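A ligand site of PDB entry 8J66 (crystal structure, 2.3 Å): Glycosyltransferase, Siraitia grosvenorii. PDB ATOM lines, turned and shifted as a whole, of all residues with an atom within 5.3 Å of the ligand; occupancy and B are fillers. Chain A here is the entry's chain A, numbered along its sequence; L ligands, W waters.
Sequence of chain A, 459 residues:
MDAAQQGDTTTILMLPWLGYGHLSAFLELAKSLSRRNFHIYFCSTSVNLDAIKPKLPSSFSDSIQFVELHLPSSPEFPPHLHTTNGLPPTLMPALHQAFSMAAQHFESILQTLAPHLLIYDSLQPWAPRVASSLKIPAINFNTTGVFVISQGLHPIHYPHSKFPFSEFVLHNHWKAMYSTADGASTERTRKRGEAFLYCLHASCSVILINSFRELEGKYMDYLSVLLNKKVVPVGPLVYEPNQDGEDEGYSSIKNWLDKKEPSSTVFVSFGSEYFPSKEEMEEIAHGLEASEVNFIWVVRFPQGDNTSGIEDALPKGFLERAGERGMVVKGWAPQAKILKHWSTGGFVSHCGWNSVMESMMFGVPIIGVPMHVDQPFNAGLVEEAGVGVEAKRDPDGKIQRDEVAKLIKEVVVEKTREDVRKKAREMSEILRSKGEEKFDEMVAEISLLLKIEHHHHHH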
ATOM      1  N   TYR A  20      13.202  -1.184  16.069  1.00  0.00           N
ATOM      2  CA  TYR A  20      12.708  -2.322  15.293  1.00  0.00           C
ATOM      3  C   TYR A  20      12.501  -1.949  13.835  1.00  0.00           C
ATOM      4  O   TYR A  20      12.841  -2.731  12.934  1.00  0.00           O
ATOM      5  CB  TYR A  20      11.408  -2.845  15.897  1.00  0.00           C
ATOM      6  CG  TYR A  20      10.852  -4.061  15.202  1.00  0.00           C
ATOM      7  CD1 TYR A  20      11.331  -5.338  15.504  1.00  0.00           C
ATOM      8  CD2 TYR A  20       9.861  -3.949  14.229  1.00  0.00           C
ATOM      9  CE1 TYR A  20      10.826  -6.454  14.856  1.00  0.00           C
ATOM     10  CE2 TYR A  20       9.356  -5.065  13.581  1.00  0.00           C
ATOM     11  CZ  TYR A  20       9.848  -6.314  13.899  1.00  0.00           C
ATOM     12  OH  TYR A  20       9.349  -7.416  13.260  1.00  0.00           O
ATOM     13  N   GLY A  21      11.939  -0.762  13.575  1.00  0.00           N
ATOM     14  CA  GLY A  21      11.751  -0.340  12.192  1.00  0.00           C
ATOM     15  C   GLY A  21      13.060  -0.186  11.444  1.00  0.00           C
ATOM     16  O   GLY A  21      13.170  -0.582  10.284  1.00  0.00           O
ATOM     17  N   HIS A  22      14.067   0.397  12.095  1.00  0.00           N
ATOM     18  CA  HIS A  22      15.385   0.517  11.482  1.00  0.00           C
ATOM     19  C   HIS A  22      16.009  -0.858  11.261  1.00  0.00           C
ATOM     20  O   HIS A  22      16.573  -1.139  10.193  1.00  0.00           O
ATOM     21  CB  HIS A  22      16.289   1.391  12.359  1.00  0.00           C
ATOM     22  CG  HIS A  22      15.823   2.810  12.462  1.00  0.00           C
ATOM     23  ND1 HIS A  22      16.597   3.871  12.056  1.00  0.00           N
ATOM     24  CD2 HIS A  22      14.665   3.341  12.919  1.00  0.00           C
ATOM     25  CE1 HIS A  22      15.932   5.005  12.268  1.00  0.00           C
ATOM     26  NE2 HIS A  22      14.761   4.702  12.792  1.00  0.00           N
ATOM     27  N   SER A  24      14.516  -3.657  10.810  1.00  0.00           N
ATOM     28  CA  SER A  24      13.752  -4.303   9.711  1.00  0.00           C
ATOM     29  C   SER A  24      14.243  -3.879   8.310  1.00  0.00           C
ATOM     30  O   SER A  24      14.323  -4.729   7.461  1.00  0.00           O
ATOM     31  CB  SER A  24      12.266  -4.138   9.925  1.00  0.00           C
ATOM     32  OG  SER A  24      11.855  -4.727  11.145  1.00  0.00           O
ATOM     33  N   LYS A  55      12.733 -13.170  11.341  1.00  0.00           N
ATOM     34  CA  LYS A  55      12.450 -12.626  10.012  1.00  0.00           C
ATOM     35  C   LYS A  55      13.451 -13.055   8.949  1.00  0.00           C
ATOM     36  O   LYS A  55      13.281 -12.707   7.777  1.00  0.00           O
ATOM     37  CB  LYS A  55      12.389 -11.094  10.077  1.00  0.00           C
ATOM     38  CG  LYS A  55      11.208 -10.590  10.900  1.00  0.00           C
ATOM     39  CD  LYS A  55      11.171  -9.078  11.078  1.00  0.00           C
ATOM     40  CE  LYS A  55      10.754  -8.361   9.810  1.00  0.00           C
ATOM     41  NZ  LYS A  55      10.470  -6.921  10.060  1.00  0.00           N
ATOM     42  N   PHE A 267      -7.061  -0.750  10.091  1.00  0.00           N
ATOM     43  CA  PHE A 267      -6.067  -1.196  11.057  1.00  0.00           C
ATOM     44  C   PHE A 267      -5.508   0.044  11.759  1.00  0.00           C
ATOM     45  O   PHE A 267      -5.190   1.034  11.103  1.00  0.00           O
ATOM     46  CB  PHE A 267      -4.963  -1.970  10.360  1.00  0.00           C
ATOM     47  CG  PHE A 267      -3.878  -2.442  11.268  1.00  0.00           C
ATOM     48  CD1 PHE A 267      -4.147  -3.301  12.320  1.00  0.00           C
ATOM     49  CD2 PHE A 267      -2.566  -2.036  11.072  1.00  0.00           C
ATOM     50  CE1 PHE A 267      -3.143  -3.737  13.153  1.00  0.00           C
ATOM     51  CE2 PHE A 267      -1.553  -2.471  11.896  1.00  0.00           C
ATOM     52  CZ  PHE A 267      -1.844  -3.326  12.947  1.00  0.00           C
ATOM     53  N   SER A 269      -2.606   1.431  14.345  1.00  0.00           N
ATOM     54  CA  SER A 269      -1.293   1.092  14.871  1.00  0.00           C
ATOM     55  C   SER A 269      -0.466   2.357  14.992  1.00  0.00           C
ATOM     56  O   SER A 269      -0.576   3.264  14.160  1.00  0.00           O
ATOM     57  CB  SER A 269      -0.570   0.078  13.987  1.00  0.00           C
ATOM     58  OG  SER A 269       0.702  -0.235  14.510  1.00  0.00           O
ATOM     59  N   PHE A 270       0.342   2.468  16.059  1.00  0.00           N
ATOM     60  CA  PHE A 270       1.229   3.602  16.237  1.00  0.00           C
ATOM     61  C   PHE A 270       2.683   3.166  16.351  1.00  0.00           C
ATOM     62  O   PHE A 270       3.512   3.878  16.926  1.00  0.00           O
ATOM     63  CB  PHE A 270       0.785   4.426  17.436  1.00  0.00           C
ATOM     64  CG  PHE A 270      -0.606   4.978  17.286  1.00  0.00           C
ATOM     65  CD1 PHE A 270      -0.837   6.080  16.491  1.00  0.00           C
ATOM     66  CD2 PHE A 270      -1.684   4.342  17.873  1.00  0.00           C
ATOM     67  CE1 PHE A 270      -2.122   6.571  16.318  1.00  0.00           C
ATOM     68  CE2 PHE A 270      -2.969   4.834  17.710  1.00  0.00           C
ATOM     69  CZ  PHE A 270      -3.181   5.946  16.933  1.00  0.00           C
ATOM     70  N   GLY A 271       3.000   2.001  15.802  1.00  0.00           N
ATOM     71  CA  GLY A 271       4.376   1.588  15.641  1.00  0.00           C
ATOM     72  C   GLY A 271       4.911   0.795  16.818  1.00  0.00           C
ATOM     73  O   GLY A 271       4.174   0.286  17.667  1.00  0.00           O
ATOM     74  N   SER A 272       6.239   0.722  16.855  1.00  0.00           N
ATOM     75  CA  SER A 272       6.942  -0.062  17.858  1.00  0.00           C
ATOM     76  C   SER A 272       7.443   0.765  19.037  1.00  0.00           C
ATOM     77  O   SER A 272       7.795   0.188  20.066  1.00  0.00           O
ATOM     78  CB  SER A 272       8.131  -0.797  17.226  1.00  0.00           C
ATOM     79  OG  SER A 272       9.138   0.127  16.835  1.00  0.00           O
ATOM     80  N   GLU A 273       7.499   2.091  18.915  1.00  0.00           N
ATOM     81  CA  GLU A 273       8.138   2.897  19.944  1.00  0.00           C
ATOM     82  C   GLU A 273       7.343   4.164  20.232  1.00  0.00           C
ATOM     83  O   GLU A 273       7.914   5.241  20.460  1.00  0.00           O
ATOM     84  CB  GLU A 273       9.575   3.251  19.562  1.00  0.00           C
ATOM     85  CG  GLU A 273       9.721   3.805  18.158  1.00  0.00           C
ATOM     86  CD  GLU A 273      11.167   4.114  17.823  1.00  0.00           C
ATOM     87  OE1 GLU A 273      11.917   3.169  17.494  1.00  0.00           O
ATOM     88  OE2 GLU A 273      11.556   5.290  17.919  1.00  0.00           O
ATOM     89  N   VAL A 298      -4.172  -2.080  17.658  1.00  0.00           N
ATOM     90  CA  VAL A 298      -3.066  -2.566  18.477  1.00  0.00           C
ATOM     91  C   VAL A 298      -2.854  -1.593  19.619  1.00  0.00           C
ATOM     92  O   VAL A 298      -2.571  -0.410  19.403  1.00  0.00           O
ATOM     93  CB  VAL A 298      -1.782  -2.711  17.646  1.00  0.00           C
ATOM     94  CG1 VAL A 298      -0.687  -3.338  18.494  1.00  0.00           C
ATOM     95  CG2 VAL A 298      -2.049  -3.544  16.425  1.00  0.00           C
ATOM     96  N   GLY A 331      -0.382  -5.759  22.505  1.00  0.00           N
ATOM     97  CA  GLY A 331       1.039  -5.978  22.308  1.00  0.00           C
ATOM     98  C   GLY A 331       1.541  -5.821  20.881  1.00  0.00           C
ATOM     99  O   GLY A 331       2.195  -4.825  20.565  1.00  0.00           O
ATOM    100  N   TRP A 332       1.247  -6.788  20.031  1.00  0.00           N
ATOM    101  CA  TRP A 332       1.814  -6.855  18.693  1.00  0.00           C
ATOM    102  C   TRP A 332       0.838  -7.568  17.766  1.00  0.00           C
ATOM    103  O   TRP A 332       0.248  -8.586  18.145  1.00  0.00           O
ATOM    104  CB  TRP A 332       3.151  -7.604  18.707  1.00  0.00           C
ATOM    105  CG  TRP A 332       4.059  -7.351  17.536  1.00  0.00           C
ATOM    106  CD1 TRP A 332       4.316  -8.192  16.503  1.00  0.00           C
ATOM    107  CD2 TRP A 332       4.858  -6.183  17.307  1.00  0.00           C
ATOM    108  NE1 TRP A 332       5.213  -7.627  15.625  1.00  0.00           N
ATOM    109  CE2 TRP A 332       5.557  -6.387  16.107  1.00  0.00           C
ATOM    110  CE3 TRP A 332       5.036  -4.979  17.997  1.00  0.00           C
ATOM    111  CZ2 TRP A 332       6.428  -5.435  15.572  1.00  0.00           C
ATOM    112  CZ3 TRP A 332       5.910  -4.034  17.473  1.00  0.00           C
ATOM    113  CH2 TRP A 332       6.587  -4.269  16.267  1.00  0.00           C
ATOM    114  N   ALA A 333       0.662  -7.033  16.569  1.00  0.00           N
ATOM    115  CA  ALA A 333      -0.227  -7.615  15.574  1.00  0.00           C
ATOM    116  C   ALA A 333       0.534  -7.945  14.298  1.00  0.00           C
ATOM    117  O   ALA A 333       1.577  -7.339  14.008  1.00  0.00           O
ATOM    118  CB  ALA A 333      -1.388  -6.669  15.240  1.00  0.00           C
ATOM    119  N   PRO A 334       0.055  -8.918  13.521  1.00  0.00           N
ATOM    120  CA  PRO A 334       0.649  -9.177  12.188  1.00  0.00           C
ATOM    121  C   PRO A 334       0.239  -8.114  11.177  1.00  0.00           C
ATOM    122  O   PRO A 334      -0.691  -8.257  10.387  1.00  0.00           O
ATOM    123  CB  PRO A 334       0.089 -10.566  11.838  1.00  0.00           C
ATOM    124  CG  PRO A 334      -1.222 -10.627  12.564  1.00  0.00           C
ATOM    125  CD  PRO A 334      -1.050  -9.845  13.833  1.00  0.00           C
ATOM    126  N   GLN A 335       0.974  -6.990  11.216  1.00  0.00           N
ATOM    127  CA  GLN A 335       0.563  -5.794  10.491  1.00  0.00           C
ATOM    128  C   GLN A 335       0.462  -6.042   8.991  1.00  0.00           C
ATOM    129  O   GLN A 335      -0.537  -5.675   8.358  1.00  0.00           O
ATOM    130  CB  GLN A 335       1.544  -4.665  10.779  1.00  0.00           C
ATOM    131  CG  GLN A 335       1.423  -3.476   9.840  1.00  0.00           C
ATOM    132  CD  GLN A 335       1.992  -2.192  10.435  1.00  0.00           C
ATOM    133  OE1 GLN A 335       1.852  -1.943  11.634  1.00  0.00           O
ATOM    134  NE2 GLN A 335       2.632  -1.385   9.599  1.00  0.00           N
ATOM    135  N   ALA A 336       1.494  -6.657   8.405  1.00  0.00           N
ATOM    136  CA  ALA A 336       1.500  -6.869   6.960  1.00  0.00           C
ATOM    137  C   ALA A 336       0.352  -7.767   6.523  1.00  0.00           C
ATOM    138  O   ALA A 336      -0.355  -7.464   5.552  1.00  0.00           O
ATOM    139  CB  ALA A 336       2.843  -7.469   6.521  1.00  0.00           C
ATOM    140  N   HIS A 350       0.453   6.004  12.606  1.00  0.00           N
ATOM    141  CA  HIS A 350       1.312   7.062  13.117  1.00  0.00           C
ATOM    142  C   HIS A 350       2.261   7.600  12.050  1.00  0.00           C
ATOM    143  O   HIS A 350       2.977   8.575  12.321  1.00  0.00           O
ATOM    144  CB  HIS A 350       2.108   6.553  14.325  1.00  0.00           C
ATOM    145  CG  HIS A 350       3.267   5.678  13.953  1.00  0.00           C
ATOM    146  ND1 HIS A 350       3.100   4.412  13.423  1.00  0.00           N
ATOM    147  CD2 HIS A 350       4.596   5.855  14.099  1.00  0.00           C
ATOM    148  CE1 HIS A 350       4.296   3.871  13.209  1.00  0.00           C
ATOM    149  NE2 HIS A 350       5.213   4.724  13.625  1.00  0.00           N
ATOM    150  N   GLY A 352       4.917   6.144  10.681  1.00  0.00           N
ATOM    151  CA  GLY A 352       6.274   5.650  10.611  1.00  0.00           C
ATOM    152  C   GLY A 352       6.596   5.164   9.219  1.00  0.00           C
ATOM    153  O   GLY A 352       5.723   4.695   8.481  1.00  0.00           O
ATOM    154  N   TRP A 353       7.872   5.288   8.848  1.00  0.00           N
ATOM    155  CA  TRP A 353       8.237   5.148   7.431  1.00  0.00           C
ATOM    156  C   TRP A 353       7.969   3.749   6.908  1.00  0.00           C
ATOM    157  O   TRP A 353       7.479   3.577   5.786  1.00  0.00           O
ATOM    158  CB  TRP A 353       9.695   5.531   7.217  1.00  0.00           C
ATOM    159  CG  TRP A 353      10.047   5.629   5.769  1.00  0.00           C
ATOM    160  CD1 TRP A 353      10.855   4.786   5.053  1.00  0.00           C
ATOM    161  CD2 TRP A 353       9.592   6.620   4.828  1.00  0.00           C
ATOM    162  NE1 TRP A 353      10.944   5.192   3.750  1.00  0.00           N
ATOM    163  CE2 TRP A 353      10.176   6.314   3.581  1.00  0.00           C
ATOM    164  CE3 TRP A 353       8.749   7.728   4.935  1.00  0.00           C
ATOM    165  CZ2 TRP A 353       9.946   7.095   2.444  1.00  0.00           C
ATOM    166  CZ3 TRP A 353       8.522   8.501   3.808  1.00  0.00           C
ATOM    167  CH2 TRP A 353       9.117   8.169   2.575  1.00  0.00           C
ATOM    168  N   ASN A 354       8.281   2.719   7.704  1.00  0.00           N
ATOM    169  CA  ASN A 354       8.016   1.351   7.248  1.00  0.00           C
ATOM    170  C   ASN A 354       6.522   1.100   7.083  1.00  0.00           C
ATOM    171  O   ASN A 354       6.102   0.408   6.148  1.00  0.00           O
ATOM    172  CB  ASN A 354       8.640   0.338   8.200  1.00  0.00           C
ATOM    173  CG  ASN A 354      10.153   0.433   8.265  1.00  0.00           C
ATOM    174  OD1 ASN A 354      10.848   0.127   7.289  1.00  0.00           O
ATOM    175  ND2 ASN A 354      10.674   0.876   9.403  1.00  0.00           N
ATOM    176  N   SER A 355       5.711   1.653   7.977  1.00  0.00           N
ATOM    177  CA  SER A 355       4.258   1.535   7.895  1.00  0.00           C
ATOM    178  C   SER A 355       3.720   2.175   6.627  1.00  0.00           C
ATOM    179  O   SER A 355       2.758   1.680   6.025  1.00  0.00           O
ATOM    180  CB  SER A 355       3.614   2.151   9.132  1.00  0.00           C
ATOM    181  OG  SER A 355       3.575   1.219  10.201  1.00  0.00           O
ATOM    182  N   VAL A 356       4.281   3.337   6.280  1.00  0.00           N
ATOM    183  CA  VAL A 356       3.866   4.029   5.065  1.00  0.00           C
ATOM    184  C   VAL A 356       4.246   3.231   3.834  1.00  0.00           C
ATOM    185  O   VAL A 356       3.450   3.078   2.903  1.00  0.00           O
ATOM    186  CB  VAL A 356       4.455   5.455   5.027  1.00  0.00           C
ATOM    187  CG1 VAL A 356       4.210   6.095   3.666  1.00  0.00           C
ATOM    188  CG2 VAL A 356       3.879   6.306   6.142  1.00  0.00           C
ATOM    189  N   GLU A 358       4.769  -0.032   3.666  1.00  0.00           N
ATOM    190  CA  GLU A 358       3.945  -1.231   3.637  1.00  0.00           C
ATOM    191  C   GLU A 358       2.557  -0.921   3.096  1.00  0.00           C
ATOM    192  O   GLU A 358       2.034  -1.641   2.236  1.00  0.00           O
ATOM    193  CB  GLU A 358       3.873  -1.843   5.038  1.00  0.00           C
ATOM    194  CG  GLU A 358       5.152  -2.540   5.469  1.00  0.00           C
ATOM    195  CD  GLU A 358       5.294  -2.642   6.973  1.00  0.00           C
ATOM    196  OE1 GLU A 358       4.294  -2.417   7.690  1.00  0.00           O
ATOM    197  OE2 GLU A 358       6.413  -2.952   7.447  1.00  0.00           O
ATOM    198  N   GLN A 375       7.375  11.658  11.528  1.00  0.00           N
ATOM    199  CA  GLN A 375       6.010  11.309  11.142  1.00  0.00           C
ATOM    200  C   GLN A 375       5.195  12.472  10.586  1.00  0.00           C
ATOM    201  O   GLN A 375       4.526  12.280   9.569  1.00  0.00           O
ATOM    202  CB  GLN A 375       5.326  10.648  12.333  1.00  0.00           C
ATOM    203  CG  GLN A 375       6.001   9.351  12.757  1.00  0.00           C
ATOM    204  CD  GLN A 375       5.905   9.084  14.244  1.00  0.00           C
ATOM    205  OE1 GLN A 375       5.004   9.586  14.914  1.00  0.00           O
ATOM    206  NE2 GLN A 375       6.845   8.306  14.770  1.00  0.00           N
HETATM  207  N1  LIG L   1       4.729  -3.605  13.436  1.00  0.00           N
HETATM  208  C1  LIG L   1       4.086  -4.828  13.449  1.00  0.00           C
HETATM  209  N2  LIG L   1       3.054  -4.957  14.352  1.00  0.00           N
HETATM  210  C2  LIG L   1       2.624  -3.984  15.239  1.00  0.00           C
HETATM  211  C3  LIG L   1       3.331  -2.745  15.163  1.00  0.00           C
HETATM  212  C4  LIG L   1       4.353  -2.584  14.295  1.00  0.00           C
HETATM  213  O1  LIG L   1       4.410  -5.747  12.707  1.00  0.00           O
HETATM  214  O2  LIG L   1       1.676  -4.217  16.004  1.00  0.00           O
HETATM  215  C5  LIG L   1       5.840  -3.408  12.502  1.00  0.00           C
HETATM  216  C6  LIG L   1       5.343  -2.648  11.219  1.00  0.00           C
HETATM  217  O3  LIG L   1       4.929  -3.571  10.213  1.00  0.00           O
HETATM  218  C7  LIG L   1       6.560  -1.899  10.778  1.00  0.00           C
HETATM  219  C8  LIG L   1       7.348  -1.670  12.072  1.00  0.00           C
HETATM  220  O4  LIG L   1       6.831  -2.582  13.092  1.00  0.00           O
HETATM  221  O5  LIG L   1       7.333  -2.703   9.886  1.00  0.00           O
HETATM  222  C9  LIG L   1       7.153  -0.268  12.528  1.00  0.00           C
HETATM  223  O6  LIG L   1       8.058   0.533  11.801  1.00  0.00           O
HETATM  224  P1  LIG L   1       7.655   2.095  11.492  1.00  0.00           P
HETATM  225  O7  LIG L   1       8.798   2.733  10.733  1.00  0.00           O
HETATM  226  O8  LIG L   1       6.393   2.159  10.678  1.00  0.00           O
HETATM  227  O9  LIG L   1       7.446   2.865  12.937  1.00  0.00           O
HETATM  228  P2  LIG L   1       8.361   2.817  14.306  1.00  0.00           P
HETATM  229  O10 LIG L   1       9.802   2.572  13.921  1.00  0.00           O
HETATM  230  O11 LIG L   1       7.888   1.703  15.200  1.00  0.00           O
HETATM  231  O12 LIG L   1       8.250   4.144  15.023  1.00  0.00           O
HETATM  232  O   HOH W   1      11.763   1.582  15.311  1.00  0.00           O
HETATM  233  O   HOH W   2       9.701   6.194  15.198  1.00  0.00           O
HETATM  234  O   HOH W   3       2.673   0.176  13.006  1.00  0.00           O
HETATM  235  O   HOH W   4      11.367   4.307  10.495  1.00  0.00           O
HETATM  236  O   HOH W   5       1.246  -0.829  17.143  1.00  0.00           O
HETATM  237  O   HOH W   6       4.449  -8.581  12.761  1.00  0.00           O
HETATM  238  O   HOH W   7       6.523   4.159  16.973  1.00  0.00           O
HETATM  239  O   HOH W   8       4.770  -6.611   9.559  1.00  0.00           O
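O of Gly 352 sits close to O8 of the ligand, 3.4 Å away. Residues that only touch the ligand: Tyr 20 (3.5 Å), Gly 21 (3.8 Å), Ser 269 (3.7 Å), Gly 271 (3.5 Å), Glu 273 (3.5 Å), Val 298 (3.5 Å) and Trp 332 (3.2 Å). Hydrophobic or aromatic side chains that line the ligand: Tyr 20, Val 298, Trp 332, Ala 333 and His 350. 16 residues have an atom within 4 Å of the ligand: Tyr 20, Gly 21, Ser 269, Gly 271, Ser 272, Glu 273, Val 298, Trp 332, Ala 333, Gln 335, His 350, Gly 352, Trp 353, Asn 354, Ser 355 and Glu 358. Along chain A the residues within 4 Å of the ligand span positions 20 to 358. The nearest printed residue that does not touch the ligand is Gln 375 (4.4 Å).
The backbone NH of Ser 272 lies within hydrogen-bond range of an oxygen (O11) of the ligand. An oxygen (O11) of the ligand lies within hydrogen-bond range of the side-chain hydroxyl of Ser 272, 2.6 Å away. N of Ser 355 is in hydrogen-bond range of O8 of the ligand. OE2 of Glu 358 sits at hydrogen-bond distance from O5 of the ligand (2.6 Å). O7 of the ligand sits at hydrogen-bond distance from N of Trp 353, at 3.3 Å. O8 of the ligand sits at hydrogen-bond distance from OG of Ser 355, at 3.0 Å. An oxygen (O7) of the ligand sits at hydrogen-bond distance from the backbone NH (N) of Asn 354 (3.1 Å). NE2 of His 350 lies within hydrogen-bond range of O9 of the ligand, 3.0 Å away. The side-chain amide nitrogen (ND2) of Asn 354 is in hydrogen-bond range of an oxygen (O7) of the ligand, 3.0 Å away. O of Ala 333 sits at hydrogen-bond distance from N2 of the ligand (2.8 Å). The backbone NH (N) of Ala 333 sits at hydrogen-bond distance from an oxygen (O2) of the ligand, 3.0 Å away. The side-chain amide nitrogen of Gln 335 is in hydrogen-bond range of an oxygen (O3) of the ligand.
Water W2 bridges O12 of the ligand (2.5 Å) and OE2 of Glu 273 (3.4 Å). Water W1 lies within hydrogen-bond range of O10 of the ligand (2.6 Å), OE1 of Glu 273 (2.7 Å), N of Gly 21 (2.9 Å), N of Tyr 20 (3.2 Å) and OG of Ser 272 (3.4 Å). Water W7 lies within hydrogen-bond range of O12 of the ligand (2.6 Å), N of Glu 273 (3.0 Å), O of Phe 270 (3.0 Å) and N of Ser 272 (3.5 Å). Water W6 lies within hydrogen-bond range of O1 of the ligand (2.8 Å), NE1 of Trp 332 (3.1 Å) and O of Ala 333 (3.4 Å). Water W8 bridges O3 of the ligand and N of Ala 336. Water W3 lies within hydrogen-bond range of the side-chain hydroxyl of Ser 269 (2.5 Å), the side-chain amide oxygen of Gln 335 (2.7 Å), the side-chain hydroxyl of Ser 355 (3.1 Å) and the backbone NH of Gly 271 (3.4 Å).
OE1 of Gln 375 lies close to O of His 350. A ring nitrogen (NE2) of His 350 lies within hydrogen-bond range of the backbone NH (N) of Gly 352, at 3.3 Å. The side-chain amide nitrogen of Gln 335 lies within hydrogen-bond range of the side-chain hydroxyl of Ser 355 (2.8 Å). The backbone carbonyl oxygen (O) of Tyr 20 sits at hydrogen-bond distance from the side-chain hydroxyl (OG) of Ser 24 (2.9 Å). The side-chain hydroxyl of Tyr 20 sits close to the side-chain amino group of Lys 55 (3.4 Å). The backbone NH of Gly 271 is in hydrogen-bond range of the side-chain hydroxyl of Ser 269. ND2 of Asn 354 sits at hydrogen-bond distance from O of Gly 21 (3.0 Å). N of His 350 is in hydrogen-bond range of O of Ser 269, at 3.3 Å.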
